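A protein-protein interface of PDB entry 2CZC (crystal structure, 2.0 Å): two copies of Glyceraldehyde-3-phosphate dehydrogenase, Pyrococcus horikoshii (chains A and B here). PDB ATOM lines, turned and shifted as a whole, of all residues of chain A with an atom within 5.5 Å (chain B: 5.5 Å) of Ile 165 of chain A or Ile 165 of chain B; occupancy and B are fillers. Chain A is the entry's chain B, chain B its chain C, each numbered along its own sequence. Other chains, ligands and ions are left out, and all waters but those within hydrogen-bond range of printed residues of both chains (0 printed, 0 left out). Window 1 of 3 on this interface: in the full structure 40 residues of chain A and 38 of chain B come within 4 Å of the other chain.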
ATOM      1  N   VAL A 163      31.062   1.972 -21.809  1.00  0.00           N
ATOM      2  CA  VAL A 163      31.472   2.656 -20.601  1.00  0.00           C
ATOM      3  C   VAL A 163      31.022   1.795 -19.422  1.00  0.00           C
ATOM      4  O   VAL A 163      29.847   1.406 -19.335  1.00  0.00           O
ATOM      5  CB  VAL A 163      30.815   4.047 -20.519  1.00  0.00           C
ATOM      6  CG1 VAL A 163      31.217   4.762 -19.221  1.00  0.00           C
ATOM      7  CG2 VAL A 163      31.220   4.861 -21.733  1.00  0.00           C
ATOM      8  N   MET A 164      31.972   1.481 -18.540  1.00  0.00           N
ATOM      9  CA  MET A 164      31.709   0.670 -17.361  1.00  0.00           C
ATOM     10  C   MET A 164      31.494   1.558 -16.132  1.00  0.00           C
ATOM     11  O   MET A 164      32.417   2.250 -15.678  1.00  0.00           O
ATOM     12  CB  MET A 164      32.882  -0.265 -17.074  1.00  0.00           C
ATOM     13  CG  MET A 164      33.456  -0.988 -18.286  1.00  0.00           C
ATOM     14  SD  MET A 164      32.456  -2.371 -18.830  1.00  0.00           S
ATOM     15  CE  MET A 164      31.146  -1.548 -19.677  1.00  0.00           C
ATOM     16  N   ILE A 165      30.276   1.554 -15.605  1.00  0.00           N
ATOM     17  CA  ILE A 165      29.992   2.313 -14.403  1.00  0.00           C
ATOM     18  C   ILE A 165      29.933   1.250 -13.319  1.00  0.00           C
ATOM     19  O   ILE A 165      28.881   0.642 -13.084  1.00  0.00           O
ATOM     20  CB  ILE A 165      28.665   3.064 -14.522  1.00  0.00           C
ATOM     21  CG1 ILE A 165      28.777   4.112 -15.633  1.00  0.00           C
ATOM     22  CG2 ILE A 165      28.318   3.738 -13.181  1.00  0.00           C
ATOM     23  CD1 ILE A 165      27.503   4.924 -15.865  1.00  0.00           C
ATOM     24  N   ARG A 166      31.071   1.021 -12.655  1.00  0.00           N
ATOM     25  CA  ARG A 166      31.153  -0.046 -11.662  1.00  0.00           C
ATOM     26  C   ARG A 166      30.943   0.273 -10.195  1.00  0.00           C
ATOM     27  O   ARG A 166      31.235   1.391  -9.737  1.00  0.00           O
ATOM     28  CB  ARG A 166      32.496  -0.763 -11.800  1.00  0.00           C
ATOM     29  CG  ARG A 166      33.425  -0.161 -12.809  1.00  0.00           C
ATOM     30  CD  ARG A 166      34.850  -0.581 -12.508  1.00  0.00           C
ATOM     31  NE  ARG A 166      34.943  -2.030 -12.329  1.00  0.00           N
ATOM     32  CZ  ARG A 166      35.370  -2.640 -11.218  1.00  0.00           C
ATOM     33  NH1 ARG A 166      35.762  -1.942 -10.159  1.00  0.00           N
ATOM     34  NH2 ARG A 166      35.391  -3.964 -11.157  1.00  0.00           N
ATOM     35  N   ARG A 167      30.441  -0.726  -9.460  1.00  0.00           N
ATOM     36  CA  ARG A 167      30.226  -0.582  -8.032  1.00  0.00           C
ATOM     37  C   ARG A 167      31.617  -0.464  -7.409  1.00  0.00           C
ATOM     38  O   ARG A 167      32.582  -0.996  -7.954  1.00  0.00           O
ATOM     39  CB  ARG A 167      29.453  -1.783  -7.432  1.00  0.00           C
ATOM     40  CG  ARG A 167      29.839  -3.178  -7.882  1.00  0.00           C
ATOM     41  CD  ARG A 167      30.506  -4.038  -6.767  1.00  0.00           C
ATOM     42  NE  ARG A 167      31.932  -3.859  -6.877  1.00  0.00           N
ATOM     43  CZ  ARG A 167      32.851  -4.812  -6.838  1.00  0.00           C
ATOM     44  NH1 ARG A 167      32.547  -6.086  -6.673  1.00  0.00           N
ATOM     45  NH2 ARG A 167      34.102  -4.460  -7.018  1.00  0.00           N
ATOM     46  N   ILE A 182      33.434  10.072  -7.694  1.00  0.00           N
ATOM     47  CA  ILE A 182      33.458   9.275  -8.917  1.00  0.00           C
ATOM     48  C   ILE A 182      34.958   9.174  -9.245  1.00  0.00           C
ATOM     49  O   ILE A 182      35.644  10.179  -9.367  1.00  0.00           O
ATOM     50  CB  ILE A 182      32.704   9.942 -10.076  1.00  0.00           C
ATOM     51  CG1 ILE A 182      31.193   9.965  -9.764  1.00  0.00           C
ATOM     52  CG2 ILE A 182      32.985   9.147 -11.393  1.00  0.00           C
ATOM     53  CD1 ILE A 182      30.385  10.778 -10.734  1.00  0.00           C
ATOM     54  N   PHE A 209      34.824   3.559 -14.712  1.00  0.00           N
ATOM     55  CA  PHE A 209      34.656   4.485 -13.604  1.00  0.00           C
ATOM     56  C   PHE A 209      34.124   3.724 -12.391  1.00  0.00           C
ATOM     57  O   PHE A 209      33.475   2.685 -12.532  1.00  0.00           O
ATOM     58  CB  PHE A 209      33.627   5.545 -13.999  1.00  0.00           C
ATOM     59  CG  PHE A 209      33.992   6.323 -15.235  1.00  0.00           C
ATOM     60  CD1 PHE A 209      34.663   7.535 -15.137  1.00  0.00           C
ATOM     61  CD2 PHE A 209      33.698   5.824 -16.505  1.00  0.00           C
ATOM     62  CE1 PHE A 209      35.046   8.239 -16.277  1.00  0.00           C
ATOM     63  CE2 PHE A 209      34.077   6.524 -17.656  1.00  0.00           C
ATOM     64  CZ  PHE A 209      34.756   7.736 -17.537  1.00  0.00           C
ATOM     65  N   VAL A 211      31.859   4.266  -8.797  1.00  0.00           N
ATOM     66  CA  VAL A 211      30.931   5.157  -8.116  1.00  0.00           C
ATOM     67  C   VAL A 211      30.495   4.504  -6.806  1.00  0.00           C
ATOM     68  O   VAL A 211      30.567   3.280  -6.655  1.00  0.00           O
ATOM     69  CB  VAL A 211      29.700   5.459  -9.005  1.00  0.00           C
ATOM     70  CG1 VAL A 211      30.170   6.024 -10.356  1.00  0.00           C
ATOM     71  CG2 VAL A 211      28.877   4.184  -9.211  1.00  0.00           C
ATOM     72  N   MET A 216      25.190  -3.477  -8.332  1.00  0.00           N
ATOM     73  CA  MET A 216      25.515  -4.003  -9.651  1.00  0.00           C
ATOM     74  C   MET A 216      26.337  -3.011 -10.461  1.00  0.00           C
ATOM     75  O   MET A 216      26.328  -1.805 -10.198  1.00  0.00           O
ATOM     76  CB  MET A 216      24.240  -4.281 -10.450  1.00  0.00           C
ATOM     77  CG  MET A 216      23.130  -4.969  -9.712  1.00  0.00           C
ATOM     78  SD  MET A 216      21.710  -5.143 -10.835  1.00  0.00           S
ATOM     79  CE  MET A 216      22.358  -6.398 -11.960  1.00  0.00           C
ATOM     80  N   HIS A 217      27.044  -3.509 -11.460  1.00  0.00           N
ATOM     81  CA  HIS A 217      27.791  -2.604 -12.317  1.00  0.00           C
ATOM     82  C   HIS A 217      26.752  -2.216 -13.384  1.00  0.00           C
ATOM     83  O   HIS A 217      25.718  -2.860 -13.479  1.00  0.00           O
ATOM     84  CB  HIS A 217      28.944  -3.321 -13.043  1.00  0.00           C
ATOM     85  CG  HIS A 217      30.056  -3.793 -12.158  1.00  0.00           C
ATOM     86  ND1 HIS A 217      30.678  -2.974 -11.238  1.00  0.00           N
ATOM     87  CD2 HIS A 217      30.717  -4.978 -12.114  1.00  0.00           C
ATOM     88  CE1 HIS A 217      31.676  -3.632 -10.670  1.00  0.00           C
ATOM     89  NE2 HIS A 217      31.722  -4.849 -11.184  1.00  0.00           N
ATOM     90  N   VAL A 218      27.025  -1.180 -14.184  1.00  0.00           N
ATOM     91  CA  VAL A 218      26.124  -0.819 -15.280  1.00  0.00           C
ATOM     92  C   VAL A 218      27.010  -0.525 -16.481  1.00  0.00           C
ATOM     93  O   VAL A 218      28.102   0.047 -16.314  1.00  0.00           O
ATOM     94  CB  VAL A 218      25.275   0.433 -14.999  1.00  0.00           C
ATOM     95  CG1 VAL A 218      24.673   0.961 -16.304  1.00  0.00           C
ATOM     96  CG2 VAL A 218      24.139   0.088 -14.030  1.00  0.00           C
ATOM     97  N   HIS A 219      26.560  -0.890 -17.666  1.00  0.00           N
ATOM     98  CA  HIS A 219      27.364  -0.637 -18.862  1.00  0.00           C
ATOM     99  C   HIS A 219      26.639   0.297 -19.823  1.00  0.00           C
ATOM    100  O   HIS A 219      25.440   0.130 -20.009  1.00  0.00           O
ATOM    101  CB  HIS A 219      27.618  -1.940 -19.657  1.00  0.00           C
ATOM    102  CG  HIS A 219      28.346  -3.011 -18.893  1.00  0.00           C
ATOM    103  ND1 HIS A 219      28.274  -4.350 -19.222  1.00  0.00           N
ATOM    104  CD2 HIS A 219      29.143  -2.936 -17.797  1.00  0.00           C
ATOM    105  CE1 HIS A 219      28.992  -5.048 -18.361  1.00  0.00           C
ATOM    106  NE2 HIS A 219      29.530  -4.216 -17.487  1.00  0.00           N
ATOM    107  N   VAL B 163      28.914  10.029 -22.318  1.00  0.00           N
ATOM    108  CA  VAL B 163      28.087   9.398 -21.304  1.00  0.00           C
ATOM    109  C   VAL B 163      28.202  10.267 -20.069  1.00  0.00           C
ATOM    110  O   VAL B 163      29.304  10.558 -19.622  1.00  0.00           O
ATOM    111  CB  VAL B 163      28.584   7.968 -20.993  1.00  0.00           C
ATOM    112  CG1 VAL B 163      27.822   7.383 -19.804  1.00  0.00           C
ATOM    113  CG2 VAL B 163      28.410   7.094 -22.213  1.00  0.00           C
ATOM    114  N   MET B 164      27.062  10.700 -19.546  1.00  0.00           N
ATOM    115  CA  MET B 164      27.027  11.533 -18.355  1.00  0.00           C
ATOM    116  C   MET B 164      26.862  10.654 -17.103  1.00  0.00           C
ATOM    117  O   MET B 164      25.850   9.980 -16.957  1.00  0.00           O
ATOM    118  CB  MET B 164      25.829  12.510 -18.399  1.00  0.00           C
ATOM    119  CG  MET B 164      25.616  13.284 -19.708  1.00  0.00           C
ATOM    120  SD  MET B 164      26.921  14.481 -20.080  1.00  0.00           S
ATOM    121  CE  MET B 164      27.907  13.532 -21.156  1.00  0.00           C
ATOM    122  N   ILE B 165      27.837  10.682 -16.198  1.00  0.00           N
ATOM    123  CA  ILE B 165      27.751   9.926 -14.940  1.00  0.00           C
ATOM    124  C   ILE B 165      27.453  11.038 -13.929  1.00  0.00           C
ATOM    125  O   ILE B 165      28.358  11.764 -13.461  1.00  0.00           O
ATOM    126  CB  ILE B 165      29.082   9.204 -14.647  1.00  0.00           C
ATOM    127  CG1 ILE B 165      29.399   8.236 -15.800  1.00  0.00           C
ATOM    128  CG2 ILE B 165      28.982   8.442 -13.333  1.00  0.00           C
ATOM    129  CD1 ILE B 165      30.825   7.669 -15.755  1.00  0.00           C
ATOM    130  N   ARG B 166      26.168  11.174 -13.597  1.00  0.00           N
ATOM    131  CA  ARG B 166      25.714  12.284 -12.753  1.00  0.00           C
ATOM    132  C   ARG B 166      25.550  12.116 -11.261  1.00  0.00           C
ATOM    133  O   ARG B 166      25.163  11.034 -10.801  1.00  0.00           O
ATOM    134  CB  ARG B 166      24.382  12.801 -13.308  1.00  0.00           C
ATOM    135  CG  ARG B 166      24.445  13.144 -14.811  1.00  0.00           C
ATOM    136  CD  ARG B 166      23.231  13.944 -15.302  1.00  0.00           C
ATOM    137  NE  ARG B 166      22.031  13.622 -14.545  1.00  0.00           N
ATOM    138  CZ  ARG B 166      21.459  14.424 -13.646  1.00  0.00           C
ATOM    139  NH1 ARG B 166      21.955  15.628 -13.385  1.00  0.00           N
ATOM    140  NH2 ARG B 166      20.411  13.990 -12.964  1.00  0.00           N
ATOM    141  N   ARG B 167      25.816  13.204 -10.523  1.00  0.00           N
ATOM    142  CA  ARG B 167      25.617  13.202  -9.072  1.00  0.00           C
ATOM    143  C   ARG B 167      24.100  13.108  -8.830  1.00  0.00           C
ATOM    144  O   ARG B 167      23.313  13.656  -9.608  1.00  0.00           O
ATOM    145  CB  ARG B 167      26.206  14.469  -8.396  1.00  0.00           C
ATOM    146  CG  ARG B 167      25.893  15.865  -8.993  1.00  0.00           C
ATOM    147  CD  ARG B 167      24.988  16.786  -8.100  1.00  0.00           C
ATOM    148  NE  ARG B 167      23.608  16.466  -8.361  1.00  0.00           N
ATOM    149  CZ  ARG B 167      22.710  17.254  -8.941  1.00  0.00           C
ATOM    150  NH1 ARG B 167      22.989  18.490  -9.330  1.00  0.00           N
ATOM    151  NH2 ARG B 167      21.523  16.746  -9.196  1.00  0.00           N
ATOM    152  N   ILE B 182      22.398   2.599  -9.204  1.00  0.00           N
ATOM    153  CA  ILE B 182      22.703   3.368 -10.394  1.00  0.00           C
ATOM    154  C   ILE B 182      21.365   3.412 -11.136  1.00  0.00           C
ATOM    155  O   ILE B 182      20.744   2.370 -11.348  1.00  0.00           O
ATOM    156  CB  ILE B 182      23.734   2.676 -11.270  1.00  0.00           C
ATOM    157  CG1 ILE B 182      25.061   2.546 -10.508  1.00  0.00           C
ATOM    158  CG2 ILE B 182      23.876   3.458 -12.585  1.00  0.00           C
ATOM    159  CD1 ILE B 182      26.145   1.780 -11.265  1.00  0.00           C
ATOM    160  N   PHE B 209      23.298   8.700 -16.648  1.00  0.00           N
ATOM    161  CA  PHE B 209      23.056   7.845 -15.514  1.00  0.00           C
ATOM    162  C   PHE B 209      23.183   8.692 -14.257  1.00  0.00           C
ATOM    163  O   PHE B 209      23.853   9.741 -14.250  1.00  0.00           O
ATOM    164  CB  PHE B 209      24.087   6.707 -15.463  1.00  0.00           C
ATOM    165  CG  PHE B 209      24.108   5.854 -16.691  1.00  0.00           C
ATOM    166  CD1 PHE B 209      24.699   6.317 -17.870  1.00  0.00           C
ATOM    167  CD2 PHE B 209      23.475   4.616 -16.700  1.00  0.00           C
ATOM    168  CE1 PHE B 209      24.646   5.562 -19.036  1.00  0.00           C
ATOM    169  CE2 PHE B 209      23.417   3.845 -17.871  1.00  0.00           C
ATOM    170  CZ  PHE B 209      23.999   4.317 -19.039  1.00  0.00           C
ATOM    171  N   VAL B 211      24.202   8.440 -10.144  1.00  0.00           N
ATOM    172  CA  VAL B 211      24.854   7.583  -9.177  1.00  0.00           C
ATOM    173  C   VAL B 211      24.875   8.274  -7.820  1.00  0.00           C
ATOM    174  O   VAL B 211      24.648   9.489  -7.730  1.00  0.00           O
ATOM    175  CB  VAL B 211      26.266   7.204  -9.634  1.00  0.00           C
ATOM    176  CG1 VAL B 211      26.194   6.630 -11.046  1.00  0.00           C
ATOM    177  CG2 VAL B 211      27.195   8.420  -9.557  1.00  0.00           C
ATOM    178  N   MET B 216      30.400  16.162  -8.010  1.00  0.00           N
ATOM    179  CA  MET B 216      30.381  16.691  -9.352  1.00  0.00           C
ATOM    180  C   MET B 216      29.972  15.596 -10.324  1.00  0.00           C
ATOM    181  O   MET B 216      29.943  14.411  -9.966  1.00  0.00           O
ATOM    182  CB  MET B 216      31.756  17.282  -9.757  1.00  0.00           C
ATOM    183  CG  MET B 216      32.920  17.071  -8.805  1.00  0.00           C
ATOM    184  SD  MET B 216      34.576  17.711  -9.344  1.00  0.00           S
ATOM    185  CE  MET B 216      34.202  18.907 -10.673  1.00  0.00           C
ATOM    186  N   HIS B 217      29.604  15.996 -11.536  1.00  0.00           N
ATOM    187  CA  HIS B 217      29.255  15.024 -12.565  1.00  0.00           C
ATOM    188  C   HIS B 217      30.562  14.640 -13.281  1.00  0.00           C
ATOM    189  O   HIS B 217      31.573  15.376 -13.209  1.00  0.00           O
ATOM    190  CB  HIS B 217      28.325  15.639 -13.626  1.00  0.00           C
ATOM    191  CG  HIS B 217      27.061  16.224 -13.082  1.00  0.00           C
ATOM    192  ND1 HIS B 217      26.119  15.471 -12.416  1.00  0.00           N
ATOM    193  CD2 HIS B 217      26.534  17.468 -13.198  1.00  0.00           C
ATOM    194  CE1 HIS B 217      25.064  16.222 -12.153  1.00  0.00           C
ATOM    195  NE2 HIS B 217      25.290  17.438 -12.618  1.00  0.00           N
ATOM    196  N   VAL B 218      30.547  13.506 -13.981  1.00  0.00           N
ATOM    197  CA  VAL B 218      31.726  13.111 -14.763  1.00  0.00           C
ATOM    198  C   VAL B 218      31.260  12.742 -16.171  1.00  0.00           C
ATOM    199  O   VAL B 218      30.194  12.135 -16.335  1.00  0.00           O
ATOM    200  CB  VAL B 218      32.462  11.909 -14.133  1.00  0.00           C
ATOM    201  CG1 VAL B 218      33.475  11.332 -15.135  1.00  0.00           C
ATOM    202  CG2 VAL B 218      33.167  12.345 -12.853  1.00  0.00           C
ATOM    203  N   HIS B 219      32.039  13.112 -17.178  1.00  0.00           N
ATOM    204  CA  HIS B 219      31.691  12.829 -18.572  1.00  0.00           C
ATOM    205  C   HIS B 219      32.667  11.868 -19.217  1.00  0.00           C
ATOM    206  O   HIS B 219      33.887  12.048 -19.085  1.00  0.00           O
ATOM    207  CB  HIS B 219      31.716  14.097 -19.430  1.00  0.00           C
ATOM    208  CG  HIS B 219      30.752  15.165 -19.001  1.00  0.00           C
ATOM    209  ND1 HIS B 219      31.030  16.513 -19.096  1.00  0.00           N
ATOM    210  CD2 HIS B 219      29.523  15.075 -18.445  1.00  0.00           C
ATOM    211  CE1 HIS B 219      30.012  17.205 -18.614  1.00  0.00           C
ATOM    212  NE2 HIS B 219      29.086  16.355 -18.215  1.00  0.00           N
ATOM    213  N   SER B 220      32.159  10.841 -19.900  1.00  0.00           N
ATOM    214  CA  SER B 220      33.051   9.932 -20.600  1.00  0.00           C
ATOM    215  C   SER B 220      32.905  10.366 -22.057  1.00  0.00           C
ATOM    216  O   SER B 220      31.871  10.109 -22.678  1.00  0.00           O
ATOM    217  CB  SER B 220      32.607   8.488 -20.416  1.00  0.00           C
ATOM    218  OG  SER B 220      33.624   7.598 -20.835  1.00  0.00           O
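Printed residues of chain A that touch a printed residue of chain B: Val 163, Ile 165, Ile 182, Phe 209, Val 211, Met 216 and Val 218.
Of the 13 printed residues of chain B, 8 touch a printed residue of chain A.
Hydrophobic or aromatic side chains of chain B within 4 Å of the printed part of chain A: Val 163, Ile 165, Ile 182, Phe 209, Val 211 and Val 218.
Ile 165 of chain A touches Ile 182 of chain B, and with the chains exchanged Ile 182 of chain A touches Ile 165 of chain B.
Ile 165 of chain A touches Phe 209 of chain B, and with the chains exchanged Phe 209 of chain A touches Ile 165 of chain B.
Ile 182 of chain A touches Val 218 of chain B, and with the chains exchanged Val 218 of chain A touches Ile 182 of chain B.
Val 211 of chain B touches its own counterpart, Val 211 of chain A.
12 positions are printed for both chains.
Val 163 of chain A touches Val 163 of chain B (CG2 to CG2, 3.6 Å).
CG2 of Val 163 of chain A touches OG of Ser 220 of chain B, 3.8 Å away.
Ile 165 of chain A touches Phe 209 of chain B.
O of Ile 165 of chain B touches CD1 of Ile 182 of chain A, at 3.5 Å.
Ile 182 of chain A touches Met 216 of chain B (CD1 to O, 3.7 Å).
Val 218 of chain B touches Ile 182 of chain A (CG2 to CG2, 3.5 Å).
CG1 of Val 218 of chain B touches CE1 of Phe 209 of chain A, 3.7 Å away.
CE2 of Phe 209 of chain A touches OG of Ser 220 of chain B, at 3.4 Å.
Ile 182 of chain B touches Met 216 of chain A.
Ile 182 of chain B touches Val 218 of chain A (CG2 to CG2, 3.7 Å).
Of chain B, only Ile 165, Ile 182 and Phe 209 come within 4 Å of Ile 165 of chain A.
Printed residues of chain B within 4 Å of Val 218 of chain A: Ile 182 (3.7 Å) and Phe 209 (3.5 Å).
His 219 of chain A touches none of the printed residues of chain B.
Printed residues of chain A within 4 Å of Ile 165 of chain B: Ile 165, Ile 182 and Phe 209.
Arg 167 of chain B touches none of the printed residues of chain A.
Of the printed residues of chain A, Val 218 of chain B touches Ile 182 and Phe 209.
Of the printed residues of chain A, Ser 220 of chain B touches Val 163 and Phe 209.
The nearest printed residue of chain A that does not touch Ile 165 of chain B is Val 211 of chain A (4.02 Å).
N of Ile 165 of chain A lies within hydrogen-bond range of O of Val 218 of chain A (2.7 Å).
The backbone carbonyl oxygen (O) of Met 164 of chain B is in hydrogen-bond range of the backbone NH (N) of Phe 209 of chain B.
N of Phe 209 of chain A is in hydrogen-bond range of O of Met 164 of chain A (2.9 Å).
N of Arg 166 of chain B is in hydrogen-bond range of O of Phe 209 of chain B.
O of Arg 166 of chain B sits at hydrogen-bond distance from N of Val 211 of chain B (2.8 Å).
The backbone NH (N) of Ile 165 of chain B is in hydrogen-bond range of the backbone carbonyl oxygen (O) of Val 218 of chain B (2.8 Å).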
